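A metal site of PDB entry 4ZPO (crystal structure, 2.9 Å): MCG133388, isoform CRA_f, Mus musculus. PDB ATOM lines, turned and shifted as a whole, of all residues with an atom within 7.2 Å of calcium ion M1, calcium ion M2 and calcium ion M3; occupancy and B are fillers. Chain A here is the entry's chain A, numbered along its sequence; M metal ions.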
ATOM      1  N   GLU A   8      -8.233   0.606   3.843  1.00  0.00           N
ATOM      2  CA  GLU A   8      -6.953  -0.106   3.828  1.00  0.00           C
ATOM      3  C   GLU A   8      -6.448  -0.337   5.246  1.00  0.00           C
ATOM      4  O   GLU A   8      -6.750   0.441   6.157  1.00  0.00           O
ATOM      5  CB  GLU A   8      -5.931   0.698   3.018  1.00  0.00           C
ATOM      6  CG  GLU A   8      -4.564   0.055   2.889  1.00  0.00           C
ATOM      7  CD  GLU A   8      -3.473   1.076   2.635  1.00  0.00           C
ATOM      8  OE1 GLU A   8      -3.801   2.264   2.455  1.00  0.00           O
ATOM      9  OE2 GLU A   8      -2.282   0.692   2.644  1.00  0.00           O
ATOM     10  N   GLU A   9      -5.697  -1.428   5.433  1.00  0.00           N
ATOM     11  CA  GLU A   9      -5.064  -1.767   6.713  1.00  0.00           C
ATOM     12  C   GLU A   9      -6.076  -2.051   7.826  1.00  0.00           C
ATOM     13  O   GLU A   9      -5.730  -2.030   9.008  1.00  0.00           O
ATOM     14  CB  GLU A   9      -4.121  -0.649   7.163  1.00  0.00           C
ATOM     15  CG  GLU A   9      -3.123  -0.198   6.117  1.00  0.00           C
ATOM     16  CD  GLU A   9      -2.073  -1.243   5.812  1.00  0.00           C
ATOM     17  OE1 GLU A   9      -1.921  -2.199   6.607  1.00  0.00           O
ATOM     18  OE2 GLU A   9      -1.396  -1.123   4.769  1.00  0.00           O
ATOM     19  N   ILE A  61      -5.256  -5.920   4.273  1.00  0.00           N
ATOM     20  CA  ILE A  61      -5.046  -5.500   2.895  1.00  0.00           C
ATOM     21  C   ILE A  61      -4.154  -4.268   2.792  1.00  0.00           C
ATOM     22  O   ILE A  61      -4.420  -3.244   3.425  1.00  0.00           O
ATOM     23  CB  ILE A  61      -6.378  -5.203   2.179  1.00  0.00           C
ATOM     24  CG1 ILE A  61      -7.242  -6.469   2.126  1.00  0.00           C
ATOM     25  CG2 ILE A  61      -6.140  -4.657   0.783  1.00  0.00           C
ATOM     26  CD1 ILE A  61      -8.614  -6.246   1.536  1.00  0.00           C
ATOM     27  N   ASP A  62      -3.107  -4.361   1.976  1.00  0.00           N
ATOM     28  CA  ASP A  62      -2.229  -3.220   1.717  1.00  0.00           C
ATOM     29  C   ASP A  62      -2.523  -2.654   0.335  1.00  0.00           C
ATOM     30  O   ASP A  62      -2.254  -3.294  -0.677  1.00  0.00           O
ATOM     31  CB  ASP A  62      -0.755  -3.641   1.826  1.00  0.00           C
ATOM     32  CG  ASP A  62       0.186  -2.457   1.740  1.00  0.00           C
ATOM     33  OD1 ASP A  62      -0.220  -1.336   2.100  1.00  0.00           O
ATOM     34  OD2 ASP A  62       1.336  -2.653   1.301  1.00  0.00           O
ATOM     35  N   ARG A  63      -3.065  -1.441   0.303  1.00  0.00           N
ATOM     36  CA  ARG A  63      -3.472  -0.828  -0.960  1.00  0.00           C
ATOM     37  C   ARG A  63      -2.282  -0.530  -1.863  1.00  0.00           C
ATOM     38  O   ARG A  63      -2.392  -0.570  -3.092  1.00  0.00           O
ATOM     39  CB  ARG A  63      -4.252   0.466  -0.705  1.00  0.00           C
ATOM     40  CG  ARG A  63      -4.978   0.995  -1.923  1.00  0.00           C
ATOM     41  CD  ARG A  63      -4.981   2.516  -1.954  1.00  0.00           C
ATOM     42  NE  ARG A  63      -3.617   3.044  -2.020  1.00  0.00           N
ATOM     43  CZ  ARG A  63      -2.960   3.259  -3.157  1.00  0.00           C
ATOM     44  NH1 ARG A  63      -1.724   3.731  -3.123  1.00  0.00           N
ATOM     45  NH2 ARG A  63      -3.539   2.991  -4.323  1.00  0.00           N
ATOM     46  N   GLU A  64      -1.142  -0.234  -1.254  1.00  0.00           N
ATOM     47  CA  GLU A  64       0.074   0.070  -2.012  1.00  0.00           C
ATOM     48  C   GLU A  64       0.625  -1.159  -2.724  1.00  0.00           C
ATOM     49  O   GLU A  64       1.273  -1.053  -3.768  1.00  0.00           O
ATOM     50  CB  GLU A  64       1.146   0.663  -1.102  1.00  0.00           C
ATOM     51  CG  GLU A  64       0.993   2.161  -0.833  1.00  0.00           C
ATOM     52  CD  GLU A  64      -0.253   2.500  -0.043  1.00  0.00           C
ATOM     53  OE1 GLU A  64      -1.108   3.238  -0.561  1.00  0.00           O
ATOM     54  OE2 GLU A  64      -0.361   2.019   1.108  1.00  0.00           O
ATOM     55  N   SER A  65       0.363  -2.337  -2.159  1.00  0.00           N
ATOM     56  CA  SER A  65       0.865  -3.582  -2.712  1.00  0.00           C
ATOM     57  C   SER A  65       0.009  -4.097  -3.863  1.00  0.00           C
ATOM     58  O   SER A  65       0.492  -4.812  -4.744  1.00  0.00           O
ATOM     59  CB  SER A  65       0.965  -4.650  -1.626  1.00  0.00           C
ATOM     60  OG  SER A  65       1.910  -4.278  -0.632  1.00  0.00           O
ATOM     61  N   LEU A  95     -10.094   1.960  -0.099  1.00  0.00           N
ATOM     62  CA  LEU A  95      -9.840   3.358   0.211  1.00  0.00           C
ATOM     63  C   LEU A  95      -8.416   3.563   0.723  1.00  0.00           C
ATOM     64  O   LEU A  95      -7.933   2.802   1.556  1.00  0.00           O
ATOM     65  CB  LEU A  95     -10.855   3.864   1.244  1.00  0.00           C
ATOM     66  CG  LEU A  95     -12.325   3.696   0.872  1.00  0.00           C
ATOM     67  CD1 LEU A  95     -13.224   4.249   1.967  1.00  0.00           C
ATOM     68  CD2 LEU A  95     -12.632   4.355  -0.461  1.00  0.00           C
ATOM     69  N   ASP A  96      -7.756   4.594   0.215  1.00  0.00           N
ATOM     70  CA  ASP A  96      -6.363   4.853   0.559  1.00  0.00           C
ATOM     71  C   ASP A  96      -6.214   5.440   1.957  1.00  0.00           C
ATOM     72  O   ASP A  96      -6.963   6.329   2.366  1.00  0.00           O
ATOM     73  CB  ASP A  96      -5.728   5.802  -0.458  1.00  0.00           C
ATOM     74  CG  ASP A  96      -4.294   6.149  -0.116  1.00  0.00           C
ATOM     75  OD1 ASP A  96      -3.573   5.277   0.410  1.00  0.00           O
ATOM     76  OD2 ASP A  96      -3.875   7.305  -0.364  1.00  0.00           O
ATOM     77  N   LEU A  97      -5.226   4.938   2.692  1.00  0.00           N
ATOM     78  CA  LEU A  97      -4.883   5.457   4.007  1.00  0.00           C
ATOM     79  C   LEU A  97      -3.530   6.154   3.931  1.00  0.00           C
ATOM     80  O   LEU A  97      -2.678   5.789   3.126  1.00  0.00           O
ATOM     81  CB  LEU A  97      -4.849   4.319   5.038  1.00  0.00           C
ATOM     82  CG  LEU A  97      -5.153   4.675   6.493  1.00  0.00           C
ATOM     83  CD1 LEU A  97      -6.569   5.197   6.633  1.00  0.00           C
ATOM     84  CD2 LEU A  97      -4.927   3.466   7.387  1.00  0.00           C
ATOM     85  N   ASN A  98      -3.334   7.172   4.770  1.00  0.00           N
ATOM     86  CA  ASN A  98      -2.068   7.910   4.757  1.00  0.00           C
ATOM     87  C   ASN A  98      -1.075   7.334   5.748  1.00  0.00           C
ATOM     88  O   ASN A  98      -0.717   7.984   6.736  1.00  0.00           O
ATOM     89  CB  ASN A  98      -2.323   9.389   5.065  1.00  0.00           C
ATOM     90  CG  ASN A  98      -1.097  10.254   4.812  1.00  0.00           C
ATOM     91  OD1 ASN A  98      -0.306   9.982   3.905  1.00  0.00           O
ATOM     92  ND2 ASN A  98      -0.930  11.297   5.613  1.00  0.00           N
ATOM     93  N   ASP A  99      -0.623   6.106   5.493  1.00  0.00           N
ATOM     94  CA  ASP A  99       0.266   5.413   6.416  1.00  0.00           C
ATOM     95  C   ASP A  99       1.684   5.288   5.870  1.00  0.00           C
ATOM     96  O   ASP A  99       2.525   4.586   6.448  1.00  0.00           O
ATOM     97  CB  ASP A  99      -0.290   4.033   6.737  1.00  0.00           C
ATOM     98  CG  ASP A  99      -0.582   3.209   5.500  1.00  0.00           C
ATOM     99  OD1 ASP A  99      -0.964   3.795   4.460  1.00  0.00           O
ATOM    100  OD2 ASP A  99      -0.429   1.971   5.561  1.00  0.00           O
ATOM    101  N   ASN A 100       1.964   5.971   4.761  1.00  0.00           N
ATOM    102  CA  ASN A 100       3.309   5.978   4.195  1.00  0.00           C
ATOM    103  C   ASN A 100       3.963   7.354   4.300  1.00  0.00           C
ATOM    104  O   ASN A 100       3.313   8.382   4.094  1.00  0.00           O
ATOM    105  CB  ASN A 100       3.279   5.534   2.727  1.00  0.00           C
ATOM    106  CG  ASN A 100       3.203   4.030   2.583  1.00  0.00           C
ATOM    107  OD1 ASN A 100       4.234   3.352   2.509  1.00  0.00           O
ATOM    108  ND2 ASN A 100       1.987   3.492   2.534  1.00  0.00           N
ATOM    109  N   SER A 101       5.244   7.365   4.632  1.00  0.00           N
ATOM    110  CA  SER A 101       5.987   8.615   4.814  1.00  0.00           C
ATOM    111  C   SER A 101       6.933   8.874   3.641  1.00  0.00           C
ATOM    112  O   SER A 101       7.510   7.927   3.094  1.00  0.00           O
ATOM    113  CB  SER A 101       6.769   8.589   6.123  1.00  0.00           C
ATOM    114  OG  SER A 101       5.910   8.363   7.228  1.00  0.00           O
ATOM    115  N   PRO A 102       7.076  10.152   3.241  1.00  0.00           N
ATOM    116  CA  PRO A 102       7.960  10.573   2.158  1.00  0.00           C
ATOM    117  C   PRO A 102       9.377  10.013   2.293  1.00  0.00           C
ATOM    118  O   PRO A 102       9.991  10.115   3.353  1.00  0.00           O
ATOM    119  CB  PRO A 102       7.966  12.091   2.292  1.00  0.00           C
ATOM    120  CG  PRO A 102       6.616  12.405   2.828  1.00  0.00           C
ATOM    121  CD  PRO A 102       6.285  11.275   3.773  1.00  0.00           C
ATOM    122  N   GLN A 129       9.667  10.319  -2.530  1.00  0.00           N
ATOM    123  CA  GLN A 129       8.614   9.417  -2.975  1.00  0.00           C
ATOM    124  C   GLN A 129       7.603   9.147  -1.867  1.00  0.00           C
ATOM    125  O   GLN A 129       7.969   9.045  -0.691  1.00  0.00           O
ATOM    126  CB  GLN A 129       9.208   8.099  -3.470  1.00  0.00           C
ATOM    127  CG  GLN A 129      10.200   8.255  -4.607  1.00  0.00           C
ATOM    128  CD  GLN A 129      10.962   6.977  -4.882  1.00  0.00           C
ATOM    129  OE1 GLN A 129      10.693   5.943  -4.273  1.00  0.00           O
ATOM    130  NE2 GLN A 129      11.915   7.044  -5.788  1.00  0.00           N
ATOM    131  N   ASP A 130       6.337   9.012  -2.248  1.00  0.00           N
ATOM    132  CA  ASP A 130       5.271   8.674  -1.313  1.00  0.00           C
ATOM    133  C   ASP A 130       4.248   7.808  -2.036  1.00  0.00           C
ATOM    134  O   ASP A 130       3.414   8.308  -2.778  1.00  0.00           O
ATOM    135  CB  ASP A 130       4.616   9.948  -0.761  1.00  0.00           C
ATOM    136  CG  ASP A 130       3.815   9.696   0.509  1.00  0.00           C
ATOM    137  OD1 ASP A 130       3.303   8.570   0.682  1.00  0.00           O
ATOM    138  OD2 ASP A 130       3.701  10.629   1.329  1.00  0.00           O
ATOM    139  N   PRO A 131       4.307   6.488  -1.793  1.00  0.00           N
ATOM    140  CA  PRO A 131       3.483   5.501  -2.514  1.00  0.00           C
ATOM    141  C   PRO A 131       1.980   5.660  -2.283  1.00  0.00           C
ATOM    142  O   PRO A 131       1.204   4.965  -2.937  1.00  0.00           O
ATOM    143  CB  PRO A 131       3.972   4.164  -1.949  1.00  0.00           C
ATOM    144  CG  PRO A 131       4.550   4.497  -0.621  1.00  0.00           C
ATOM    145  CD  PRO A 131       5.169   5.847  -0.786  1.00  0.00           C
ATOM    146  N   ASP A 132       1.584   6.562  -1.396  1.00  0.00           N
ATOM    147  CA  ASP A 132       0.162   6.837  -1.189  1.00  0.00           C
ATOM    148  C   ASP A 132      -0.424   7.571  -2.384  1.00  0.00           C
ATOM    149  O   ASP A 132       0.314   8.025  -3.262  1.00  0.00           O
ATOM    150  CB  ASP A 132      -0.050   7.628   0.107  1.00  0.00           C
ATOM    151  CG  ASP A 132       0.210   6.803   1.348  1.00  0.00           C
ATOM    152  OD1 ASP A 132       0.134   5.552   1.264  1.00  0.00           O
ATOM    153  OD2 ASP A 132       0.472   7.391   2.424  1.00  0.00           O
ATOM    154  N   VAL A 133      -1.741   7.708  -2.408  1.00  0.00           N
ATOM    155  CA  VAL A 133      -2.430   8.233  -3.594  1.00  0.00           C
ATOM    156  C   VAL A 133      -3.374   9.375  -3.256  1.00  0.00           C
ATOM    157  O   VAL A 133      -4.107   9.336  -2.266  1.00  0.00           O
ATOM    158  CB  VAL A 133      -3.207   7.097  -4.305  1.00  0.00           C
ATOM    159  CG1 VAL A 133      -4.361   7.643  -5.147  1.00  0.00           C
ATOM    160  CG2 VAL A 133      -2.263   6.267  -5.159  1.00  0.00           C
ATOM    161  N   THR A 135      -4.110  13.179  -2.163  1.00  0.00           N
ATOM    162  CA  THR A 135      -3.476  14.227  -1.377  1.00  0.00           C
ATOM    163  C   THR A 135      -2.480  13.631  -0.399  1.00  0.00           C
ATOM    164  O   THR A 135      -1.619  14.324   0.132  1.00  0.00           O
ATOM    165  CB  THR A 135      -4.519  15.063  -0.602  1.00  0.00           C
ATOM    166  OG1 THR A 135      -5.212  14.221   0.330  1.00  0.00           O
ATOM    167  CG2 THR A 135      -5.529  15.689  -1.560  1.00  0.00           C
ATOM    168  N   ASN A 136      -2.582  12.315  -0.183  1.00  0.00           N
ATOM    169  CA  ASN A 136      -1.738  11.630   0.780  1.00  0.00           C
ATOM    170  C   ASN A 136      -0.298  11.447   0.305  1.00  0.00           C
ATOM    171  O   ASN A 136       0.565  11.008   1.075  1.00  0.00           O
ATOM    172  CB  ASN A 136      -2.345  10.262   1.129  1.00  0.00           C
ATOM    173  CG  ASN A 136      -3.674  10.375   1.840  1.00  0.00           C
ATOM    174  OD1 ASN A 136      -3.937  11.359   2.532  1.00  0.00           O
ATOM    175  ND2 ASN A 136      -4.530   9.375   1.672  1.00  0.00           N
ATOM    176  N   THR A 137      -0.038  11.772  -0.951  1.00  0.00           N
ATOM    177  CA  THR A 137       1.324  11.705  -1.487  1.00  0.00           C
ATOM    178  C   THR A 137       2.029  13.041  -1.279  1.00  0.00           C
ATOM    179  O   THR A 137       1.436  13.986  -0.757  1.00  0.00           O
ATOM    180  CB  THR A 137       1.327  11.339  -2.986  1.00  0.00           C
ATOM    181  OG1 THR A 137       2.680  11.150  -3.424  1.00  0.00           O
ATOM    182  CG2 THR A 137       0.684  12.442  -3.805  1.00  0.00           C
ATOM    183  N   VAL A 138       3.295  13.106  -1.688  1.00  0.00           N
ATOM    184  CA  VAL A 138       4.140  14.292  -1.503  1.00  0.00           C
ATOM    185  C   VAL A 138       3.446  15.583  -1.946  1.00  0.00           C
ATOM    186  O   VAL A 138       2.952  15.681  -3.063  1.00  0.00           O
ATOM    187  CB  VAL A 138       5.471  14.156  -2.282  1.00  0.00           C
ATOM    188  CG1 VAL A 138       6.277  15.444  -2.196  1.00  0.00           C
ATOM    189  CG2 VAL A 138       6.272  12.983  -1.748  1.00  0.00           C
ATOM    190  N   ASP A 187       3.883  15.371   2.845  1.00  0.00           N
ATOM    191  CA  ASP A 187       2.689  15.012   2.094  1.00  0.00           C
ATOM    192  C   ASP A 187       1.513  15.874   2.546  1.00  0.00           C
ATOM    193  O   ASP A 187       1.659  16.730   3.411  1.00  0.00           O
ATOM    194  CB  ASP A 187       2.361  13.518   2.247  1.00  0.00           C
ATOM    195  CG  ASP A 187       2.185  13.087   3.702  1.00  0.00           C
ATOM    196  OD1 ASP A 187       1.402  13.735   4.442  1.00  0.00           O
ATOM    197  OD2 ASP A 187       2.814  12.091   4.100  1.00  0.00           O
ATOM    198  N   GLY A 188       0.339  15.644   1.949  1.00  0.00           N
ATOM    199  CA  GLY A 188      -0.832  16.438   2.252  1.00  0.00           C
ATOM    200  C   GLY A 188      -1.906  15.665   2.996  1.00  0.00           C
ATOM    201  O   GLY A 188      -3.080  15.711   2.625  1.00  0.00           O
ATOM    202  N   GLY A 189      -1.511  14.950   4.032  1.00  0.00           N
ATOM    203  CA  GLY A 189      -2.453  14.209   4.860  1.00  0.00           C
ATOM    204  C   GLY A 189      -2.690  14.899   6.187  1.00  0.00           C
ATOM    205  O   GLY A 189      -2.015  15.861   6.524  1.00  0.00           O
ATOM    206  N   ARG A 193       2.842  13.721   7.137  1.00  0.00           N
ATOM    207  CA  ARG A 193       4.023  12.918   7.426  1.00  0.00           C
ATOM    208  C   ARG A 193       5.190  13.407   6.568  1.00  0.00           C
ATOM    209  O   ARG A 193       4.981  13.874   5.447  1.00  0.00           O
ATOM    210  CB  ARG A 193       3.755  11.440   7.163  1.00  0.00           C
ATOM    211  CG  ARG A 193       2.344  11.017   7.561  1.00  0.00           C
ATOM    212  CD  ARG A 193       2.077   9.567   7.189  1.00  0.00           C
ATOM    213  NE  ARG A 193       2.614   8.639   8.172  1.00  0.00           N
ATOM    214  CZ  ARG A 193       1.883   8.073   9.136  1.00  0.00           C
ATOM    215  NH1 ARG A 193       0.594   8.325   9.229  1.00  0.00           N
ATOM    216  NH2 ARG A 193       2.459   7.232   9.987  1.00  0.00           N
HETATM  217 CA    CA M   1      -1.823   3.935   1.808  1.00  0.00          CA
HETATM  218 CA    CA M   2       1.794   9.597   2.685  1.00  0.00          CA
HETATM  219 CA    CA M   3       0.029   0.720   3.335  1.00  0.00          CA
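OE2 of Glu 64 lies close to ND2 of Asn 100 (3.1 Å). OG of Ser 65 is in hydrogen-bond range of OD2 of Asp 62 (2.6 Å). The backbone carbonyl oxygen (O) of Leu 95 is in hydrogen-bond range of the backbone NH (N) of Glu 8 (3.2 Å). The backbone carbonyl oxygen of Asn 98 is in hydrogen-bond range of the guanidinium group of Arg 193 (2.8 Å). NE of Arg 63 lies close to OD1 of Asp 96, 3.3 Å away. OD2 of Asp 96 lies within hydrogen-bond range of N of Val 133 (3.0 Å). N of Glu 9 is in hydrogen-bond range of O of Ile 61. The backbone NH (N) of Gly 189 sits at hydrogen-bond distance from the side-chain carboxylate (OD1) of Asp 187, at 3.2 Å.
The nearest printed residue that does not touch calcium ion M1 is Arg 63 (4.3 Å).
Within 4 Å of calcium ion M2: Asn 98, Asn 100, Asp 130, Asp 132, Asn 136 and Asp 187. Along chain A the residues within 4 Å of calcium ion M2 span positions 98 to 187. The nearest printed residue that does not touch calcium ion M2 is Arg 193 (4.5 Å).
Of the 28 residues printed, 6 come within 4 Å of calcium ion M3. The nearest printed residue that does not touch calcium ion M3 is Arg 63 (4.8 Å).
Calcium ion M1 is bound by O of Leu 97 (2.4 Å), OE2 of Glu 64 (2.5 Å), OE1 of Glu 64 (2.6 Å), OD1 of Asp 132 (2.6 Å), OD1 of Asp 96 (2.6 Å), OE1 of Glu 8 (2.7 Å) and OD1 of Asp 99 (2.8 Å).
Calcium ion M2 is bound by the backbone carbonyl oxygen (O) of Asn 100 (2.4 Å), the side-chain amide oxygen (OD1) of Asn 98 (2.5 Å), the backbone carbonyl oxygen (O) of Asn 136 (2.5 Å), the side-chain carboxylate (OD2) of Asp 130 (2.6 Å), the side-chain carboxylate (OD2) of Asp 132 (2.6 Å) and the side-chain carboxylate (OD1) of Asp 130 (2.7 Å). Calcium ion M2 has six donor atoms within binding distance. Slightly farther from calcium ion M2 lies OD2 of Asp 187 (3.0 Å).
OD1 of Asp 62 binds calcium ion M3 (2.4 Å). Calcium ion M3 is bound by OE2 of Glu 8, at 2.4 Å. The side-chain carboxylate (OD2) of Asp 99 binds calcium ion M3 (2.6 Å). Calcium ion M3 is bound by OE2 of Glu 64. The side-chain carboxylate (OE2) of Glu 9 is bound to calcium ion M3 (2.7 Å). Calcium ion M3 has five donor atoms within binding distance.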
